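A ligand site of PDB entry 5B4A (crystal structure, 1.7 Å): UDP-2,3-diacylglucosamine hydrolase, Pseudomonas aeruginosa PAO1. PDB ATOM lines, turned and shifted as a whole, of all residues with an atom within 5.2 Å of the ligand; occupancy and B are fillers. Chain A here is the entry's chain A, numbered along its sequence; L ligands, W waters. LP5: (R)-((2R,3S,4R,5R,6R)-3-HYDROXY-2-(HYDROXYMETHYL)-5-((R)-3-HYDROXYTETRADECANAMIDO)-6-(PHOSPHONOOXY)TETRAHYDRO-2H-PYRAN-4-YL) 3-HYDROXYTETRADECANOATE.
NE of Arg 80 lies within salt-bridge range of O48 of the ligand (2.8 Å). O4 of the ligand lies within hydrogen-bond range of OG1 of Thr 164. An oxygen (O43) of the ligand lies within hydrogen-bond range of the side-chain amino group (NZ) of Lys 167, at 2.8 Å. O6 of the ligand lies within hydrogen-bond range of NE2 of His 195 (2.8 Å). The side-chain carboxylate (OD2) of Asp 122 lies within hydrogen-bond range of an oxygen (O4) of the ligand, 3.3 Å away. An oxygen (O48) of the ligand is in hydrogen-bond range of the side-chain amide nitrogen of Asn 79, at 2.9 Å. An oxygen (O46) of the ligand lies within hydrogen-bond range of the side-chain hydroxyl (OG) of Ser 160 (2.6 Å). NH1 of Arg 157 is in salt-bridge range of O46 of the ligand (2.7 Å).
The side-chain carboxylate of Glu 159 is in salt-bridge range of the side-chain amino group of Lys 155, 3.0 Å away. The side-chain amide oxygen (OD1) of Asn 79 is in hydrogen-bond range of a ring nitrogen (ND1) of His 195, 3.1 Å away. The backbone NH (N) of Trp 46 lies within hydrogen-bond range of the backbone carbonyl oxygen (O) of Arg 80, 3.1 Å away. The backbone carbonyl oxygen (O) of His 195 lies close to a ring nitrogen (NE2) of His 197 (3.2 Å). O of Ser 160 is in hydrogen-bond range of OG1 of Thr 164 (2.9 Å). The backbone NH (N) of Tyr 125 sits at hydrogen-bond distance from the side-chain carboxylate (OD1) of Asp 122 (3.4 Å). The backbone carbonyl oxygen of Leu 141 sits close to the guanidinium group of Arg 149. The side-chain carboxylate (OD1) of Asp 122 lies within salt-bridge range of the side-chain amino group (NZ) of Lys 167 (2.9 Å).
Merely in contact with the ligand: Trp 46, Ile 47, Phe 82, Leu 83, Ala 124, Tyr 125, Leu 128, Leu 141, Arg 149, Ala 153, Lys 155, Leu 156, Glu 159 and Gln 163. 22 residues have an atom within 4 Å of the ligand: Trp 46, Ile 47, Asn 79, Arg 80, Phe 82, Leu 83, Asp 122, Ala 124, Tyr 125, Leu 128, Leu 141, Arg 149, Ala 153, Lys 155, Leu 156, Arg 157, Glu 159, Ser 160, Gln 163, Thr 164, Lys 167 and His 195. The nearest printed residue that does not touch the ligand is Ile 172 (4.1 Å).
Water W5 lies within hydrogen-bond range of an oxygen (O6) of the ligand (2.6 Å), the side-chain carboxylate (OD2) of Asp 122 (2.6 Å) and the backbone carbonyl oxygen (O) of Ile 172 (3.1 Å). Water W4 lies within hydrogen-bond range of O47 of the ligand and ND2 of Asn 79. Water W3 lies within hydrogen-bond range of OE1 of Gln 163 and O43 of the ligand. Water W2 bridges the backbone carbonyl oxygen (O) of Asn 79 and an oxygen (O7) of the ligand. Water W6 bridges O of His 195 (2.7 Å) and O5 of the ligand (3.5 Å).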
ATOM      1  N   ALA A  45       9.547  25.985  14.048  1.00  0.00           N
ATOM      2  CA  ALA A  45       8.303  25.847  14.796  1.00  0.00           C
ATOM      3  C   ALA A  45       7.268  26.744  14.130  1.00  0.00           C
ATOM      4  O   ALA A  45       7.597  27.720  13.456  1.00  0.00           O
ATOM      5  CB  ALA A  45       8.482  26.196  16.279  1.00  0.00           C
ATOM      6  N   TRP A  46       6.015  26.402  14.320  1.00  0.00           N
ATOM      7  CA  TRP A  46       4.920  27.260  13.847  1.00  0.00           C
ATOM      8  C   TRP A  46       3.812  27.247  14.874  1.00  0.00           C
ATOM      9  O   TRP A  46       3.329  26.173  15.252  1.00  0.00           O
ATOM     10  CB  TRP A  46       4.370  26.777  12.507  1.00  0.00           C
ATOM     11  CG  TRP A  46       3.615  27.789  11.704  1.00  0.00           C
ATOM     12  CD1 TRP A  46       2.246  27.891  11.560  1.00  0.00           C
ATOM     13  CD2 TRP A  46       4.175  28.802  10.882  1.00  0.00           C
ATOM     14  NE1 TRP A  46       1.941  28.903  10.679  1.00  0.00           N
ATOM     15  CE2 TRP A  46       3.112  29.487  10.266  1.00  0.00           C
ATOM     16  CE3 TRP A  46       5.491  29.184  10.599  1.00  0.00           C
ATOM     17  CZ2 TRP A  46       3.324  30.539   9.393  1.00  0.00           C
ATOM     18  CZ3 TRP A  46       5.682  30.238   9.726  1.00  0.00           C
ATOM     19  CH2 TRP A  46       4.616  30.883   9.130  1.00  0.00           C
ATOM     20  N   ILE A  47       3.357  28.440  15.293  1.00  0.00           N
ATOM     21  CA  ILE A  47       2.287  28.524  16.270  1.00  0.00           C
ATOM     22  C   ILE A  47       0.940  28.846  15.640  1.00  0.00           C
ATOM     23  O   ILE A  47      -0.069  28.881  16.344  1.00  0.00           O
ATOM     24  CB  ILE A  47       2.582  29.545  17.389  1.00  0.00           C
ATOM     25  CG1 ILE A  47       2.831  30.946  16.846  1.00  0.00           C
ATOM     26  CG2 ILE A  47       3.742  29.106  18.247  1.00  0.00           C
ATOM     27  CD1 ILE A  47       2.405  32.016  17.852  1.00  0.00           C
ATOM     28  N   ASN A  79       6.241  17.713  11.982  1.00  0.00           N
ATOM     29  CA  ASN A  79       5.911  17.785  13.403  1.00  0.00           C
ATOM     30  C   ASN A  79       6.198  19.157  13.997  1.00  0.00           C
ATOM     31  O   ASN A  79       5.645  19.485  15.048  1.00  0.00           O
ATOM     32  CB  ASN A  79       6.703  16.742  14.159  1.00  0.00           C
ATOM     33  CG  ASN A  79       8.174  16.848  13.901  1.00  0.00           C
ATOM     34  OD1 ASN A  79       8.648  16.646  12.779  1.00  0.00           O
ATOM     35  ND2 ASN A  79       8.923  17.144  14.946  1.00  0.00           N
ATOM     36  N   ARG A  80       7.035  19.977  13.357  1.00  0.00           N
ATOM     37  CA  ARG A  80       7.308  21.322  13.841  1.00  0.00           C
ATOM     38  C   ARG A  80       6.298  22.337  13.366  1.00  0.00           C
ATOM     39  O   ARG A  80       6.103  23.363  14.049  1.00  0.00           O
ATOM     40  CB  ARG A  80       8.669  21.797  13.381  1.00  0.00           C
ATOM     41  CG  ARG A  80       9.825  20.951  13.815  1.00  0.00           C
ATOM     42  CD  ARG A  80      10.052  20.946  15.307  1.00  0.00           C
ATOM     43  NE  ARG A  80      11.322  20.283  15.585  1.00  0.00           N
ATOM     44  CZ  ARG A  80      12.507  20.849  15.475  1.00  0.00           C
ATOM     45  NH1 ARG A  80      12.649  22.132  15.151  1.00  0.00           N
ATOM     46  NH2 ARG A  80      13.590  20.127  15.723  1.00  0.00           N
ATOM     47  N   PHE A  82       2.957  21.734  11.627  1.00  0.00           N
ATOM     48  CA  PHE A  82       1.638  21.219  11.242  1.00  0.00           C
ATOM     49  C   PHE A  82       0.541  22.261  11.387  1.00  0.00           C
ATOM     50  O   PHE A  82      -0.565  22.019  10.881  1.00  0.00           O
ATOM     51  CB  PHE A  82       1.284  19.944  12.064  1.00  0.00           C
ATOM     52  CG  PHE A  82       1.241  20.169  13.541  1.00  0.00           C
ATOM     53  CD1 PHE A  82       2.387  20.033  14.302  1.00  0.00           C
ATOM     54  CD2 PHE A  82       0.050  20.530  14.157  1.00  0.00           C
ATOM     55  CE1 PHE A  82       2.384  20.280  15.647  1.00  0.00           C
ATOM     56  CE2 PHE A  82       0.026  20.774  15.524  1.00  0.00           C
ATOM     57  CZ  PHE A  82       1.183  20.644  16.277  1.00  0.00           C
ATOM     58  N   LEU A  83       0.798  23.415  11.989  1.00  0.00           N
ATOM     59  CA  LEU A  83      -0.189  24.463  12.094  1.00  0.00           C
ATOM     60  C   LEU A  83      -0.149  25.447  10.921  1.00  0.00           C
ATOM     61  O   LEU A  83      -0.936  26.399  10.925  1.00  0.00           O
ATOM     62  CB  LEU A  83      -0.034  25.236  13.407  1.00  0.00           C
ATOM     63  CG  LEU A  83      -0.399  24.406  14.656  1.00  0.00           C
ATOM     64  CD1 LEU A  83      -0.122  25.220  15.881  1.00  0.00           C
ATOM     65  CD2 LEU A  83      -1.838  23.950  14.624  1.00  0.00           C
ATOM     66  N   CYS A 119       7.010   6.286  12.531  1.00  0.00           N
ATOM     67  CA  CYS A 119       7.886   5.980  13.652  1.00  0.00           C
ATOM     68  C   CYS A 119       7.060   5.402  14.816  1.00  0.00           C
ATOM     69  O   CYS A 119       6.970   5.959  15.915  1.00  0.00           O
ATOM     70  CB  CYS A 119       8.670   7.220  14.070  1.00  0.00           C
ATOM     71  SG  CYS A 119       9.738   7.836  12.758  1.00  0.00           S
ATOM     72  N   ASP A 122       8.092   4.523  18.591  1.00  0.00           N
ATOM     73  CA  ASP A 122       8.331   5.637  19.514  1.00  0.00           C
ATOM     74  C   ASP A 122       6.997   5.973  20.166  1.00  0.00           C
ATOM     75  O   ASP A 122       6.281   6.886  19.767  1.00  0.00           O
ATOM     76  CB  ASP A 122       8.918   6.820  18.747  1.00  0.00           C
ATOM     77  CG  ASP A 122       9.436   7.914  19.657  1.00  0.00           C
ATOM     78  OD1 ASP A 122       9.113   7.876  20.857  1.00  0.00           O
ATOM     79  OD2 ASP A 122      10.121   8.810  19.104  1.00  0.00           O
ATOM     80  N   ALA A 124       6.032   7.145  23.058  1.00  0.00           N
ATOM     81  CA  ALA A 124       5.821   8.449  23.662  1.00  0.00           C
ATOM     82  C   ALA A 124       5.516   9.494  22.605  1.00  0.00           C
ATOM     83  O   ALA A 124       4.666  10.365  22.822  1.00  0.00           O
ATOM     84  CB  ALA A 124       7.039   8.867  24.484  1.00  0.00           C
ATOM     85  N   TYR A 125       6.202   9.428  21.459  1.00  0.00           N
ATOM     86  CA  TYR A 125       5.930  10.383  20.399  1.00  0.00           C
ATOM     87  C   TYR A 125       4.586  10.094  19.756  1.00  0.00           C
ATOM     88  O   TYR A 125       3.831  11.008  19.444  1.00  0.00           O
ATOM     89  CB  TYR A 125       7.046  10.386  19.351  1.00  0.00           C
ATOM     90  CG  TYR A 125       6.616  11.282  18.225  1.00  0.00           C
ATOM     91  CD1 TYR A 125       6.433  12.634  18.465  1.00  0.00           C
ATOM     92  CD2 TYR A 125       6.287  10.786  16.988  1.00  0.00           C
ATOM     93  CE1 TYR A 125       5.960  13.469  17.491  1.00  0.00           C
ATOM     94  CE2 TYR A 125       5.803  11.612  15.994  1.00  0.00           C
ATOM     95  CZ  TYR A 125       5.641  12.966  16.262  1.00  0.00           C
ATOM     96  OH  TYR A 125       5.139  13.819  15.300  1.00  0.00           O
ATOM     97  N   LEU A 128       2.013  11.742  21.870  1.00  0.00           N
ATOM     98  CA  LEU A 128       2.033  13.193  21.706  1.00  0.00           C
ATOM     99  C   LEU A 128       1.384  13.605  20.401  1.00  0.00           C
ATOM    100  O   LEU A 128       0.576  14.545  20.357  1.00  0.00           O
ATOM    101  CB  LEU A 128       3.477  13.703  21.766  1.00  0.00           C
ATOM    102  CG  LEU A 128       3.680  15.206  21.525  1.00  0.00           C
ATOM    103  CD1 LEU A 128       2.978  15.989  22.613  1.00  0.00           C
ATOM    104  CD2 LEU A 128       5.117  15.545  21.480  1.00  0.00           C
ATOM    105  N   LEU A 132      -1.688  16.137  19.829  1.00  0.00           N
ATOM    106  CA  LEU A 132      -1.463  17.413  19.139  1.00  0.00           C
ATOM    107  C   LEU A 132      -2.392  17.587  17.953  1.00  0.00           C
ATOM    108  O   LEU A 132      -2.807  18.712  17.630  1.00  0.00           O
ATOM    109  CB  LEU A 132      -0.018  17.491  18.658  1.00  0.00           C
ATOM    110  CG  LEU A 132       1.017  17.963  19.649  1.00  0.00           C
ATOM    111  CD1 LEU A 132       2.394  17.765  19.041  1.00  0.00           C
ATOM    112  CD2 LEU A 132       0.796  19.412  20.048  1.00  0.00           C
ATOM    113  N   LEU A 141      -5.747  25.251  21.298  1.00  0.00           N
ATOM    114  CA  LEU A 141      -4.465  25.921  21.057  1.00  0.00           C
ATOM    115  C   LEU A 141      -4.648  27.243  20.330  1.00  0.00           C
ATOM    116  O   LEU A 141      -3.968  28.236  20.656  1.00  0.00           O
ATOM    117  CB  LEU A 141      -3.518  25.013  20.264  1.00  0.00           C
ATOM    118  CG  LEU A 141      -2.924  23.792  20.950  1.00  0.00           C
ATOM    119  CD1 LEU A 141      -2.078  23.033  19.926  1.00  0.00           C
ATOM    120  CD2 LEU A 141      -2.084  24.181  22.158  1.00  0.00           C
ATOM    121  N   ARG A 149       1.185  30.692  23.259  1.00  0.00           N
ATOM    122  CA  ARG A 149       1.524  29.657  22.287  1.00  0.00           C
ATOM    123  C   ARG A 149       3.024  29.504  22.148  1.00  0.00           C
ATOM    124  O   ARG A 149       3.523  28.374  22.119  1.00  0.00           O
ATOM    125  CB  ARG A 149       0.895  29.952  20.932  1.00  0.00           C
ATOM    126  CG  ARG A 149      -0.522  29.416  20.853  1.00  0.00           C
ATOM    127  CD  ARG A 149      -1.143  29.595  19.485  1.00  0.00           C
ATOM    128  NE  ARG A 149      -1.968  30.784  19.467  1.00  0.00           N
ATOM    129  CZ  ARG A 149      -2.266  31.472  18.378  1.00  0.00           C
ATOM    130  NH1 ARG A 149      -1.795  31.148  17.187  1.00  0.00           N
ATOM    131  NH2 ARG A 149      -3.039  32.541  18.510  1.00  0.00           N
ATOM    132  N   LEU A 152       4.239  27.495  25.097  1.00  0.00           N
ATOM    133  CA  LEU A 152       4.026  26.060  25.051  1.00  0.00           C
ATOM    134  C   LEU A 152       4.871  25.415  23.962  1.00  0.00           C
ATOM    135  O   LEU A 152       5.344  24.294  24.139  1.00  0.00           O
ATOM    136  CB  LEU A 152       2.539  25.762  24.885  1.00  0.00           C
ATOM    137  CG  LEU A 152       1.623  26.400  25.977  1.00  0.00           C
ATOM    138  CD1 LEU A 152       0.235  25.716  25.988  1.00  0.00           C
ATOM    139  CD2 LEU A 152       2.194  26.424  27.434  1.00  0.00           C
ATOM    140  N   ALA A 153       5.128  26.131  22.860  1.00  0.00           N
ATOM    141  CA  ALA A 153       6.025  25.597  21.834  1.00  0.00           C
ATOM    142  C   ALA A 153       7.436  25.431  22.384  1.00  0.00           C
ATOM    143  O   ALA A 153       8.101  24.414  22.135  1.00  0.00           O
ATOM    144  CB  ALA A 153       6.026  26.505  20.600  1.00  0.00           C
ATOM    145  N   LYS A 155       8.207  24.911  25.513  1.00  0.00           N
ATOM    146  CA  LYS A 155       8.162  23.795  26.447  1.00  0.00           C
ATOM    147  C   LYS A 155       8.176  22.450  25.726  1.00  0.00           C
ATOM    148  O   LYS A 155       8.872  21.521  26.149  1.00  0.00           O
ATOM    149  CB  LYS A 155       6.925  23.928  27.351  1.00  0.00           C
ATOM    150  CG  LYS A 155       6.619  22.723  28.255  1.00  0.00           C
ATOM    151  CD  LYS A 155       7.666  22.440  29.289  1.00  0.00           C
ATOM    152  CE  LYS A 155       7.147  21.493  30.365  1.00  0.00           C
ATOM    153  NZ  LYS A 155       8.213  21.106  31.333  1.00  0.00           N
ATOM    154  N   LEU A 156       7.422  22.325  24.623  1.00  0.00           N
ATOM    155  CA  LEU A 156       7.476  21.091  23.850  1.00  0.00           C
ATOM    156  C   LEU A 156       8.850  20.866  23.246  1.00  0.00           C
ATOM    157  O   LEU A 156       9.339  19.738  23.231  1.00  0.00           O
ATOM    158  CB  LEU A 156       6.422  21.101  22.746  1.00  0.00           C
ATOM    159  CG  LEU A 156       4.974  20.995  23.181  1.00  0.00           C
ATOM    160  CD1 LEU A 156       4.088  21.211  21.966  1.00  0.00           C
ATOM    161  CD2 LEU A 156       4.680  19.635  23.841  1.00  0.00           C
ATOM    162  N   ARG A 157       9.491  21.929  22.744  1.00  0.00           N
ATOM    163  CA  ARG A 157      10.832  21.757  22.191  1.00  0.00           C
ATOM    164  C   ARG A 157      11.804  21.307  23.271  1.00  0.00           C
ATOM    165  O   ARG A 157      12.676  20.458  23.021  1.00  0.00           O
ATOM    166  CB  ARG A 157      11.351  23.058  21.561  1.00  0.00           C
ATOM    167  CG  ARG A 157      10.601  23.550  20.312  1.00  0.00           C
ATOM    168  CD  ARG A 157      10.860  22.675  19.043  1.00  0.00           C
ATOM    169  NE  ARG A 157      12.289  22.544  18.753  1.00  0.00           N
ATOM    170  CZ  ARG A 157      12.989  21.413  18.797  1.00  0.00           C
ATOM    171  NH1 ARG A 157      12.396  20.258  19.082  1.00  0.00           N
ATOM    172  NH2 ARG A 157      14.293  21.442  18.547  1.00  0.00           N
ATOM    173  N   GLU A 159      11.208  19.621  26.145  1.00  0.00           N
ATOM    174  CA  GLU A 159      10.997  18.230  26.521  1.00  0.00           C
ATOM    175  C   GLU A 159      11.402  17.276  25.401  1.00  0.00           C
ATOM    176  O   GLU A 159      11.918  16.174  25.646  1.00  0.00           O
ATOM    177  CB  GLU A 159       9.536  18.001  26.888  1.00  0.00           C
ATOM    178  CG  GLU A 159       9.128  18.795  28.087  1.00  0.00           C
ATOM    179  CD  GLU A 159       9.944  18.473  29.318  1.00  0.00           C
ATOM    180  OE1 GLU A 159      10.239  17.263  29.519  1.00  0.00           O
ATOM    181  OE2 GLU A 159      10.286  19.417  30.067  1.00  0.00           O
ATOM    182  N   SER A 160      11.175  17.672  24.156  1.00  0.00           N
ATOM    183  CA  SER A 160      11.581  16.845  23.019  1.00  0.00           C
ATOM    184  C   SER A 160      13.105  16.727  22.946  1.00  0.00           C
ATOM    185  O   SER A 160      13.654  15.641  22.688  1.00  0.00           O
ATOM    186  CB  SER A 160      11.031  17.450  21.728  1.00  0.00           C
ATOM    187  OG  SER A 160      11.379  16.650  20.596  1.00  0.00           O
ATOM    188  N   ARG A 161      13.804  17.830  23.193  1.00  0.00           N
ATOM    189  CA  ARG A 161      15.265  17.778  23.192  1.00  0.00           C
ATOM    190  C   ARG A 161      15.797  16.901  24.313  1.00  0.00           C
ATOM    191  O   ARG A 161      16.750  16.160  24.125  1.00  0.00           O
ATOM    192  CB  ARG A 161      15.849  19.198  23.272  1.00  0.00           C
ATOM    193  CG  ARG A 161      15.632  19.950  21.908  1.00  0.00           C
ATOM    194  CD  ARG A 161      15.854  21.474  21.985  1.00  0.00           C
ATOM    195  NE  ARG A 161      17.213  21.799  22.215  1.00  0.00           N
ATOM    196  CZ  ARG A 161      17.739  22.271  23.357  1.00  0.00           C
ATOM    197  NH1 ARG A 161      16.941  22.574  24.376  1.00  0.00           N
ATOM    198  NH2 ARG A 161      19.040  22.402  23.536  1.00  0.00           N
ATOM    199  N   GLN A 163      14.102  14.331  25.803  1.00  0.00           N
ATOM    200  CA  GLN A 163      13.680  12.950  25.585  1.00  0.00           C
ATOM    201  C   GLN A 163      14.363  12.304  24.387  1.00  0.00           C
ATOM    202  O   GLN A 163      14.759  11.138  24.451  1.00  0.00           O
ATOM    203  CB  GLN A 163      12.165  12.889  25.410  1.00  0.00           C
ATOM    204  CG  GLN A 163      11.365  13.242  26.643  1.00  0.00           C
ATOM    205  CD  GLN A 163      11.602  12.309  27.794  1.00  0.00           C
ATOM    206  OE1 GLN A 163      11.430  11.113  27.680  1.00  0.00           O
ATOM    207  NE2 GLN A 163      11.994  12.865  28.929  1.00  0.00           N
ATOM    208  N   THR A 164      14.490  13.030  23.273  1.00  0.00           N
ATOM    209  CA  THR A 164      15.096  12.422  22.087  1.00  0.00           C
ATOM    210  C   THR A 164      16.526  11.973  22.360  1.00  0.00           C
ATOM    211  O   THR A 164      16.975  10.946  21.841  1.00  0.00           O
ATOM    212  CB  THR A 164      15.023  13.394  20.911  1.00  0.00           C
ATOM    213  OG1 THR A 164      13.624  13.642  20.599  1.00  0.00           O
ATOM    214  CG2 THR A 164      15.701  12.809  19.684  1.00  0.00           C
ATOM    215  N   LYS A 167      16.601   8.268  23.670  1.00  0.00           N
ATOM    216  CA  LYS A 167      16.005   7.172  22.905  1.00  0.00           C
ATOM    217  C   LYS A 167      17.021   6.492  21.987  1.00  0.00           C
ATOM    218  O   LYS A 167      17.902   7.124  21.420  1.00  0.00           O
ATOM    219  CB  LYS A 167      14.841   7.683  22.052  1.00  0.00           C
ATOM    220  CG  LYS A 167      13.693   8.377  22.822  1.00  0.00           C
ATOM    221  CD  LYS A 167      12.675   8.961  21.855  1.00  0.00           C
ATOM    222  CE  LYS A 167      11.632   9.711  22.586  1.00  0.00           C
ATOM    223  NZ  LYS A 167      10.551  10.251  21.733  1.00  0.00           N
ATOM    224  N   ILE A 172      13.544   5.627  17.325  1.00  0.00           N
ATOM    225  CA  ILE A 172      13.113   6.857  16.704  1.00  0.00           C
ATOM    226  C   ILE A 172      13.061   6.800  15.186  1.00  0.00           C
ATOM    227  O   ILE A 172      12.458   7.681  14.581  1.00  0.00           O
ATOM    228  CB  ILE A 172      13.974   8.062  17.125  1.00  0.00           C
ATOM    229  CG1 ILE A 172      15.408   7.900  16.661  1.00  0.00           C
ATOM    230  CG2 ILE A 172      13.919   8.256  18.628  1.00  0.00           C
ATOM    231  CD1 ILE A 172      16.214   9.212  16.834  1.00  0.00           C
ATOM    232  N   HIS A 195      12.023  13.727   8.091  1.00  0.00           N
ATOM    233  CA  HIS A 195      11.871  13.548   9.532  1.00  0.00           C
ATOM    234  C   HIS A 195      13.046  12.864  10.230  1.00  0.00           C
ATOM    235  O   HIS A 195      13.480  13.328  11.297  1.00  0.00           O
ATOM    236  CB  HIS A 195      10.595  12.805   9.919  1.00  0.00           C
ATOM    237  CG  HIS A 195      10.388  12.780  11.398  1.00  0.00           C
ATOM    238  ND1 HIS A 195      10.063  13.917  12.121  1.00  0.00           N
ATOM    239  CD2 HIS A 195      10.545  11.800  12.308  1.00  0.00           C
ATOM    240  CE1 HIS A 195      10.009  13.628  13.395  1.00  0.00           C
ATOM    241  NE2 HIS A 195      10.277  12.357  13.548  1.00  0.00           N
ATOM    242  N   HIS A 197      16.281  12.371   9.406  1.00  0.00           N
ATOM    243  CA  HIS A 197      17.620  12.972   9.329  1.00  0.00           C
ATOM    244  C   HIS A 197      18.695  11.960   8.917  1.00  0.00           C
ATOM    245  O   HIS A 197      19.848  12.082   9.309  1.00  0.00           O
ATOM    246  CB  HIS A 197      18.053  13.606  10.652  1.00  0.00           C
ATOM    247  CG  HIS A 197      17.058  14.585  11.194  1.00  0.00           C
ATOM    248  ND1 HIS A 197      17.250  15.239  12.394  1.00  0.00           N
ATOM    249  CD2 HIS A 197      15.884  15.024  10.700  1.00  0.00           C
ATOM    250  CE1 HIS A 197      16.210  16.015  12.629  1.00  0.00           C
ATOM    251  NE2 HIS A 197      15.369  15.904  11.620  1.00  0.00           N
HETATM  252  O48 LP5 L   1      10.958  17.821  16.850  1.00  0.00           O
HETATM  253  P45 LP5 L   1      12.249  17.128  17.346  1.00  0.00           P
HETATM  254  O46 LP5 L   1      12.838  17.591  18.722  1.00  0.00           O
HETATM  255  O47 LP5 L   1      13.247  17.045  16.278  1.00  0.00           O
HETATM  256  O1  LP5 L   1      11.775  15.612  17.739  1.00  0.00           O
HETATM  257  C1  LP5 L   1      10.651  14.961  17.160  1.00  0.00           C
HETATM  258  C2  LP5 L   1       9.649  14.662  18.264  1.00  0.00           C
HETATM  259  N2  LP5 L   1       9.231  15.894  18.941  1.00  0.00           N
HETATM  260  C7  LP5 L   1       8.250  16.667  18.497  1.00  0.00           C
HETATM  261  C8  LP5 L   1       7.938  17.931  19.267  1.00  0.00           C
HETATM  262  C16 LP5 L   1       8.208  19.178  18.444  1.00  0.00           C
HETATM  263  O44 LP5 L   1       9.614  19.394  18.480  1.00  0.00           O
HETATM  264  C17 LP5 L   1       7.529  20.406  19.080  1.00  0.00           C
HETATM  265  C18 LP5 L   1       7.256  21.470  18.026  1.00  0.00           C
HETATM  266  C19 LP5 L   1       6.458  22.633  18.581  1.00  0.00           C
HETATM  267  C20 LP5 L   1       5.727  23.410  17.487  1.00  0.00           C
HETATM  268  C21 LP5 L   1       4.215  23.237  17.541  1.00  0.00           C
HETATM  269  C22 LP5 L   1       3.633  23.988  18.736  1.00  0.00           C
HETATM  270  C23 LP5 L   1       2.196  23.600  18.995  1.00  0.00           C
HETATM  271  C24 LP5 L   1       1.733  23.979  20.379  1.00  0.00           C
HETATM  272  C25 LP5 L   1       2.023  25.434  20.734  1.00  0.00           C
HETATM  273  C26 LP5 L   1       1.531  26.403  19.685  1.00  0.00           C
HETATM  274  C27 LP5 L   1       0.085  26.250  19.342  1.00  0.00           C
HETATM  275  O7  LP5 L   1       7.593  16.372  17.521  1.00  0.00           O
HETATM  276  C3  LP5 L   1      10.295  13.737  19.267  1.00  0.00           C
HETATM  277  C4  LP5 L   1      10.811  12.488  18.582  1.00  0.00           C
HETATM  278  C5  LP5 L   1      11.729  12.873  17.426  1.00  0.00           C
HETATM  279  O5  LP5 L   1      11.092  13.768  16.527  1.00  0.00           O
HETATM  280  C6  LP5 L   1      12.135  11.645  16.663  1.00  0.00           C
HETATM  281  O6  LP5 L   1      10.949  11.221  15.977  1.00  0.00           O
HETATM  282  O4  LP5 L   1      11.569  11.708  19.511  1.00  0.00           O
HETATM  283  O3  LP5 L   1       9.262  13.363  20.161  1.00  0.00           O
HETATM  284  C28 LP5 L   1       9.536  13.455  21.553  1.00  0.00           C
HETATM  285  O42 LP5 L   1      10.687  13.547  21.985  1.00  0.00           O
HETATM  286  C29 LP5 L   1       8.324  13.435  22.406  1.00  0.00           C
HETATM  287  C30 LP5 L   1       8.581  12.896  23.782  1.00  0.00           C
HETATM  288  O43 LP5 L   1       8.964  11.517  23.633  1.00  0.00           O
HETATM  289  C31 LP5 L   1       7.359  13.096  24.663  1.00  0.00           C
HETATM  290  C32 LP5 L   1       7.150  14.576  25.037  1.00  0.00           C
HETATM  291  C33 LP5 L   1       5.908  14.880  25.883  1.00  0.00           C
HETATM  292  C34 LP5 L   1       6.049  16.338  26.321  1.00  0.00           C
HETATM  293  C35 LP5 L   1       5.010  16.863  27.296  1.00  0.00           C
HETATM  294  C36 LP5 L   1       5.231  18.362  27.455  1.00  0.00           C
HETATM  295  C37 LP5 L   1       4.048  19.164  27.990  1.00  0.00           C
HETATM  296  C38 LP5 L   1       4.127  19.401  29.484  1.00  0.00           C
HETATM  297  C39 LP5 L   1       2.946  18.757  30.190  1.00  0.00           C
HETATM  298  C40 LP5 L   1       2.814  19.230  31.637  1.00  0.00           C
HETATM  299  C41 LP5 L   1       1.683  18.483  32.305  1.00  0.00           C
HETATM  300  O   HOH W   1      15.544  16.857  19.373  1.00  0.00           O
HETATM  301  O   HOH W   2       5.213  17.764  17.137  1.00  0.00           O
HETATM  302  O   HOH W   3       9.595  10.275  25.990  1.00  0.00           O
HETATM  303  O   HOH W   4      11.773  16.609  14.196  1.00  0.00           O
HETATM  304  O   HOH W   5      10.322   8.772  16.470  1.00  0.00           O
HETATM  305  O   HOH W   6      13.290  14.044  13.870  1.00  0.00           O
